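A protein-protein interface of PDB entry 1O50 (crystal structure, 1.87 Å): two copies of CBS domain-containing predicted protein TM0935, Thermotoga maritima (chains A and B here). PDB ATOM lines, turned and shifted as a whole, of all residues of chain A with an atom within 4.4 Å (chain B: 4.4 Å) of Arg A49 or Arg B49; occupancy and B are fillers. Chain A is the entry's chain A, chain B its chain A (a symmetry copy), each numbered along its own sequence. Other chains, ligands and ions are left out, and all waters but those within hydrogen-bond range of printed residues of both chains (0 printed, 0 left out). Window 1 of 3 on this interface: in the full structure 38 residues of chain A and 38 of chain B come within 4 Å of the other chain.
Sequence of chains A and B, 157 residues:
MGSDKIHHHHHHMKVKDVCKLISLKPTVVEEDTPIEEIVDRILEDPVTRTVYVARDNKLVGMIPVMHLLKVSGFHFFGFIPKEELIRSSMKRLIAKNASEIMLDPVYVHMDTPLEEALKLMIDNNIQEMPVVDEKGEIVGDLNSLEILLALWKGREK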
ATOM      1  N   PRO A  46       2.450 -29.261 -30.573  1.00  0.00           N
ATOM      2  CA  PRO A  46       2.758 -27.846 -30.360  1.00  0.00           C
ATOM      3  C   PRO A  46       2.542 -27.246 -28.953  1.00  0.00           C
ATOM      4  O   PRO A  46       2.930 -26.110 -28.736  1.00  0.00           O
ATOM      5  CB  PRO A  46       1.899 -27.143 -31.446  1.00  0.00           C
ATOM      6  CG  PRO A  46       0.876 -28.080 -31.844  1.00  0.00           C
ATOM      7  CD  PRO A  46       1.413 -29.435 -31.595  1.00  0.00           C
ATOM      8  N   VAL A  47       1.980 -28.013 -28.033  1.00  0.00           N
ATOM      9  CA  VAL A  47       1.911 -27.685 -26.618  1.00  0.00           C
ATOM     10  C   VAL A  47       3.307 -27.732 -26.001  1.00  0.00           C
ATOM     11  O   VAL A  47       3.559 -27.153 -24.921  1.00  0.00           O
ATOM     12  CB  VAL A  47       0.885 -28.679 -25.885  1.00  0.00           C
ATOM     13  CG1 VAL A  47       1.429 -30.073 -25.690  1.00  0.00           C
ATOM     14  CG2 VAL A  47       0.375 -28.123 -24.588  1.00  0.00           C
ATOM     15  N   THR A  48       4.227 -28.389 -26.709  1.00  0.00           N
ATOM     16  CA  THR A  48       5.525 -28.704 -26.190  1.00  0.00           C
ATOM     17  C   THR A  48       6.236 -27.399 -25.957  1.00  0.00           C
ATOM     18  O   THR A  48       6.237 -26.546 -26.823  1.00  0.00           O
ATOM     19  CB  THR A  48       6.300 -29.505 -27.215  1.00  0.00           C
ATOM     20  OG1 THR A  48       5.725 -30.800 -27.401  1.00  0.00           O
ATOM     21  CG2 THR A  48       7.686 -29.823 -26.756  1.00  0.00           C
ATOM     22  N   ARG A  49       6.851 -27.256 -24.793  1.00  0.00           N
ATOM     23  CA  ARG A  49       7.521 -26.003 -24.439  1.00  0.00           C
ATOM     24  C   ARG A  49       8.985 -26.214 -24.112  1.00  0.00           C
ATOM     25  O   ARG A  49       9.784 -25.249 -24.136  1.00  0.00           O
ATOM     26  CB  ARG A  49       6.751 -25.264 -23.317  1.00  0.00           C
ATOM     27  CG  ARG A  49       5.503 -24.515 -23.844  1.00  0.00           C
ATOM     28  CD  ARG A  49       4.498 -24.312 -22.746  1.00  0.00           C
ATOM     29  NE  ARG A  49       3.467 -23.328 -23.038  1.00  0.00           N
ATOM     30  CZ  ARG A  49       2.307 -23.567 -23.594  1.00  0.00           C
ATOM     31  NH1 ARG A  49       1.988 -24.783 -24.033  1.00  0.00           N
ATOM     32  NH2 ARG A  49       1.446 -22.563 -23.713  1.00  0.00           N
ATOM     33  N   THR A  50       9.336 -27.445 -23.802  1.00  0.00           N
ATOM     34  CA  THR A  50      10.712 -27.834 -23.553  1.00  0.00           C
ATOM     35  C   THR A  50      10.951 -29.236 -24.163  1.00  0.00           C
ATOM     36  O   THR A  50      10.177 -30.189 -23.905  1.00  0.00           O
ATOM     37  CB  THR A  50      11.057 -27.840 -22.040  1.00  0.00           C
ATOM     38  OG1 THR A  50      10.743 -26.571 -21.411  1.00  0.00           O
ATOM     39  CG2 THR A  50      12.589 -27.979 -21.849  1.00  0.00           C
ATOM     40  N   PRO A  64      14.629 -25.536 -24.028  1.00  0.00           N
ATOM     41  CA  PRO A  64      13.433 -24.682 -24.040  1.00  0.00           C
ATOM     42  C   PRO A  64      13.199 -24.039 -25.408  1.00  0.00           C
ATOM     43  O   PRO A  64      14.127 -23.619 -26.120  1.00  0.00           O
ATOM     44  CB  PRO A  64      13.779 -23.607 -22.999  1.00  0.00           C
ATOM     45  CG  PRO A  64      14.670 -24.263 -22.139  1.00  0.00           C
ATOM     46  CD  PRO A  64      15.600 -25.075 -23.013  1.00  0.00           C
ATOM     47  N   VAL A  65      11.933 -23.958 -25.805  1.00  0.00           N
ATOM     48  CA  VAL A  65      11.640 -23.400 -27.102  1.00  0.00           C
ATOM     49  C   VAL A  65      12.181 -21.972 -27.228  1.00  0.00           C
ATOM     50  O   VAL A  65      12.594 -21.566 -28.319  1.00  0.00           O
ATOM     51  CB  VAL A  65      10.161 -23.426 -27.371  1.00  0.00           C
ATOM     52  CG1 VAL A  65       9.816 -22.552 -28.608  1.00  0.00           C
ATOM     53  CG2 VAL A  65       9.736 -24.854 -27.570  1.00  0.00           C
ATOM     54  N   GLN A 127       8.798 -23.211 -19.104  1.00  0.00           N
ATOM     55  CA  GLN A 127       7.419 -23.574 -18.797  1.00  0.00           C
ATOM     56  C   GLN A 127       7.109 -25.085 -18.892  1.00  0.00           C
ATOM     57  O   GLN A 127       5.936 -25.492 -18.989  1.00  0.00           O
ATOM     58  CB  GLN A 127       6.478 -22.768 -19.702  1.00  0.00           C
ATOM     59  CG  GLN A 127       6.638 -21.274 -19.470  1.00  0.00           C
ATOM     60  CD  GLN A 127       5.570 -20.436 -20.062  1.00  0.00           C
ATOM     61  OE1 GLN A 127       4.422 -20.789 -19.989  1.00  0.00           O
ATOM     62  NE2 GLN A 127       5.934 -19.254 -20.582  1.00  0.00           N
ATOM     63  N   GLU A 128       8.140 -25.929 -18.880  1.00  0.00           N
ATOM     64  CA  GLU A 128       7.930 -27.390 -18.934  1.00  0.00           C
ATOM     65  C   GLU A 128       9.197 -28.013 -18.451  1.00  0.00           C
ATOM     66  O   GLU A 128      10.298 -27.615 -18.848  1.00  0.00           O
ATOM     67  CB  GLU A 128       7.635 -27.898 -20.332  1.00  0.00           C
ATOM     68  CG  GLU A 128       7.186 -29.343 -20.384  1.00  0.00           C
ATOM     69  CD  GLU A 128       6.931 -29.886 -21.770  1.00  0.00           C
ATOM     70  OE1 GLU A 128       7.039 -29.139 -22.725  1.00  0.00           O
ATOM     71  OE2 GLU A 128       6.585 -31.087 -21.918  1.00  0.00           O
ATOM     72  N   LEU A 145       0.876 -24.793 -17.434  1.00  0.00           N
ATOM     73  CA  LEU A 145      -0.552 -24.783 -17.508  1.00  0.00           C
ATOM     74  C   LEU A 145      -1.138 -25.644 -16.385  1.00  0.00           C
ATOM     75  O   LEU A 145      -2.186 -25.328 -15.845  1.00  0.00           O
ATOM     76  CB  LEU A 145      -1.030 -25.285 -18.883  1.00  0.00           C
ATOM     77  CG  LEU A 145      -0.389 -24.688 -20.151  1.00  0.00           C
ATOM     78  CD1 LEU A 145      -1.195 -25.142 -21.368  1.00  0.00           C
ATOM     79  CD2 LEU A 145      -0.261 -23.186 -20.112  1.00  0.00           C
ATOM     80  N   PRO B  46      -4.416 -25.238 -25.489  1.00  0.00           N
ATOM     81  CA  PRO B  46      -3.153 -25.173 -24.752  1.00  0.00           C
ATOM     82  C   PRO B  46      -1.872 -24.770 -25.514  1.00  0.00           C
ATOM     83  O   PRO B  46      -0.849 -24.578 -24.877  1.00  0.00           O
ATOM     84  CB  PRO B  46      -3.052 -26.591 -24.124  1.00  0.00           C
ATOM     85  CG  PRO B  46      -3.934 -27.449 -24.879  1.00  0.00           C
ATOM     86  CD  PRO B  46      -4.994 -26.585 -25.444  1.00  0.00           C
ATOM     87  N   VAL B  47      -1.955 -24.612 -26.825  1.00  0.00           N
ATOM     88  CA  VAL B  47      -0.914 -24.023 -27.651  1.00  0.00           C
ATOM     89  C   VAL B  47      -0.779 -22.534 -27.342  1.00  0.00           C
ATOM     90  O   VAL B  47       0.257 -21.900 -27.642  1.00  0.00           O
ATOM     91  CB  VAL B  47      -1.235 -24.298 -29.199  1.00  0.00           C
ATOM     92  CG1 VAL B  47      -2.357 -23.449 -29.744  1.00  0.00           C
ATOM     93  CG2 VAL B  47      -0.017 -24.187 -30.067  1.00  0.00           C
ATOM     94  N   THR B  48      -1.812 -21.983 -26.702  1.00  0.00           N
ATOM     95  CA  THR B  48      -1.942 -20.568 -26.514  1.00  0.00           C
ATOM     96  C   THR B  48      -0.806 -20.134 -25.629  1.00  0.00           C
ATOM     97  O   THR B  48      -0.558 -20.752 -24.612  1.00  0.00           O
ATOM     98  CB  THR B  48      -3.249 -20.269 -25.811  1.00  0.00           C
ATOM     99  OG1 THR B  48      -4.367 -20.568 -26.650  1.00  0.00           O
ATOM    100  CG2 THR B  48      -3.425 -18.811 -25.537  1.00  0.00           C
ATOM    101  N   ARG B  49      -0.131 -19.061 -26.012  1.00  0.00           N
ATOM    102  CA  ARG B  49       1.032 -18.588 -25.258  1.00  0.00           C
ATOM    103  C   ARG B  49       0.867 -17.154 -24.798  1.00  0.00           C
ATOM    104  O   ARG B  49       1.570 -16.703 -23.865  1.00  0.00           O
ATOM    105  CB  ARG B  49       2.339 -18.822 -26.055  1.00  0.00           C
ATOM    106  CG  ARG B  49       2.822 -20.290 -25.990  1.00  0.00           C
ATOM    107  CD  ARG B  49       3.695 -20.618 -27.168  1.00  0.00           C
ATOM    108  NE  ARG B  49       4.477 -21.837 -27.027  1.00  0.00           N
ATOM    109  CZ  ARG B  49       4.109 -23.037 -27.396  1.00  0.00           C
ATOM    110  NH1 ARG B  49       2.892 -23.268 -27.886  1.00  0.00           N
ATOM    111  NH2 ARG B  49       4.981 -24.031 -27.270  1.00  0.00           N
ATOM    112  N   THR B  50      -0.036 -16.442 -25.441  1.00  0.00           N
ATOM    113  CA  THR B  50      -0.383 -15.083 -25.068  1.00  0.00           C
ATOM    114  C   THR B  50      -1.908 -14.894 -25.237  1.00  0.00           C
ATOM    115  O   THR B  50      -2.480 -15.208 -26.309  1.00  0.00           O
ATOM    116  CB  THR B  50       0.387 -14.028 -25.907  1.00  0.00           C
ATOM    117  OG1 THR B  50       1.821 -14.242 -25.858  1.00  0.00           O
ATOM    118  CG2 THR B  50       0.201 -12.621 -25.283  1.00  0.00           C
ATOM    119  N   PRO B  64       0.843 -12.537 -21.481  1.00  0.00           N
ATOM    120  CA  PRO B  64       1.686 -13.725 -21.684  1.00  0.00           C
ATOM    121  C   PRO B  64       1.515 -14.749 -20.561  1.00  0.00           C
ATOM    122  O   PRO B  64       1.379 -14.423 -19.369  1.00  0.00           O
ATOM    123  CB  PRO B  64       3.104 -13.137 -21.656  1.00  0.00           C
ATOM    124  CG  PRO B  64       2.917 -11.818 -22.090  1.00  0.00           C
ATOM    125  CD  PRO B  64       1.665 -11.310 -21.411  1.00  0.00           C
ATOM    126  N   VAL B  65       1.511 -16.025 -20.931  1.00  0.00           N
ATOM    127  CA  VAL B  65       1.315 -17.046 -19.931  1.00  0.00           C
ATOM    128  C   VAL B  65       2.379 -16.960 -18.832  1.00  0.00           C
ATOM    129  O   VAL B  65       2.086 -17.253 -17.669  1.00  0.00           O
ATOM    130  CB  VAL B  65       1.315 -18.412 -20.556  1.00  0.00           C
ATOM    131  CG1 VAL B  65       1.420 -19.512 -19.465  1.00  0.00           C
ATOM    132  CG2 VAL B  65       0.062 -18.564 -21.373  1.00  0.00           C
ATOM    133  N   GLN B 127       6.088 -15.415 -26.760  1.00  0.00           N
ATOM    134  CA  GLN B 127       6.104 -16.335 -27.892  1.00  0.00           C
ATOM    135  C   GLN B 127       4.825 -16.321 -28.758  1.00  0.00           C
ATOM    136  O   GLN B 127       4.564 -17.265 -29.529  1.00  0.00           O
ATOM    137  CB  GLN B 127       6.398 -17.751 -27.378  1.00  0.00           C
ATOM    138  CG  GLN B 127       7.754 -17.818 -26.693  1.00  0.00           C
ATOM    139  CD  GLN B 127       8.256 -19.188 -26.443  1.00  0.00           C
ATOM    140  OE1 GLN B 127       8.129 -20.036 -27.288  1.00  0.00           O
ATOM    141  NE2 GLN B 127       8.924 -19.398 -25.299  1.00  0.00           N
ATOM    142  N   GLU B 128       4.010 -15.274 -28.640  1.00  0.00           N
ATOM    143  CA  GLU B 128       2.783 -15.167 -29.455  1.00  0.00           C
ATOM    144  C   GLU B 128       2.379 -13.730 -29.416  1.00  0.00           C
ATOM    145  O   GLU B 128       2.375 -13.095 -28.355  1.00  0.00           O
ATOM    146  CB  GLU B 128       1.641 -16.013 -28.927  1.00  0.00           C
ATOM    147  CG  GLU B 128       0.455 -16.106 -29.864  1.00  0.00           C
ATOM    148  CD  GLU B 128      -0.715 -16.905 -29.340  1.00  0.00           C
ATOM    149  OE1 GLU B 128      -0.615 -17.457 -28.260  1.00  0.00           O
ATOM    150  OE2 GLU B 128      -1.759 -17.014 -30.034  1.00  0.00           O
ATOM    151  N   LEU B 145       6.553 -20.856 -32.942  1.00  0.00           N
ATOM    152  CA  LEU B 145       6.683 -22.090 -33.655  1.00  0.00           C
ATOM    153  C   LEU B 145       6.631 -21.828 -35.163  1.00  0.00           C
ATOM    154  O   LEU B 145       7.304 -22.499 -35.930  1.00  0.00           O
ATOM    155  CB  LEU B 145       5.578 -23.079 -33.237  1.00  0.00           C
ATOM    156  CG  LEU B 145       5.324 -23.311 -31.734  1.00  0.00           C
ATOM    157  CD1 LEU B 145       4.382 -24.504 -31.576  1.00  0.00           C
ATOM    158  CD2 LEU B 145       6.586 -23.504 -30.933  1.00  0.00           C
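O of Pro A46 lies within hydrogen-bond range of NH1 of Arg B49 (3.0 Å).
The backbone carbonyl oxygen (O) of Thr A48 sits at hydrogen-bond distance from the guanidinium group (NH2) of Arg B49 (2.8 Å).
The guanidinium group of Arg A49 sits at hydrogen-bond distance from the backbone carbonyl oxygen of Pro B46, 3.0 Å away.
NH2 of Arg A49 is in hydrogen-bond range of O of Thr B48.
O of Val A47 sits at hydrogen-bond distance from NH1 of Arg A49 (3.0 Å).
The backbone carbonyl oxygen (O) of Arg A49 lies within hydrogen-bond range of the backbone NH (N) of Val A65.
The backbone NH (N) of Arg A49 is in hydrogen-bond range of the side-chain carboxylate (OE1) of Glu A128, at 2.8 Å.
The guanidinium group of Arg B49 lies within hydrogen-bond range of the backbone carbonyl oxygen of Val B47 (3.0 Å).
O of Arg B49 is in hydrogen-bond range of N of Val B65 (3.0 Å).
OE1 of Glu B128 lies within hydrogen-bond range of N of Arg B49 (2.8 Å).
Among the printed residues, pairs that only touch across the chains: Gln A127 with Val B65, Val A65 with Gln B127, Arg A49 with Arg B49, Leu A145 with Pro B46, Pro A46 with Leu B145, Val A47 with Pro B46 and Pro A46 with Val B47.
Arg B49 touches just these residues of chain A: Pro A46, Thr A48 and Arg A49.
Of the printed residues of chain A, Thr B48 touches Arg A49.
Of the printed residues of chain B, Val A47 touches Pro B46 (3.8 Å).
Printed residues of chain B within 4 Å of Gln A127: Val B65.
Of the printed residues of chain A, Val B65 touches Gln A127.
Printed residues of chain B within 4 Å of Val A65: Gln B127.
Pro B64 touches none of the printed residues of chain A.
Printed residues of chain A that touch a printed residue of chain B: Pro A46, Val A47, Thr A48, Arg A49, Val A65, Gln A127 and Leu A145.
Pro A46 touches Leu B145, and with the chains exchanged Leu A145 touches Pro B46.
Thr A48 touches Arg B49, and with the chains exchanged Arg A49 touches Thr B48.
Arg B49 touches its own counterpart, Arg A49.
Val A65 touches Gln B127, and with the chains exchanged Gln A127 touches Val B65.
Positions printed for both chains: 46, 47, 48, 49, 50, 64, 65, 127, 128 and 145.
Of the 11 pairs that touch across the chains among the printed residues, 11 have their exchanged pair printed and touching as well.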
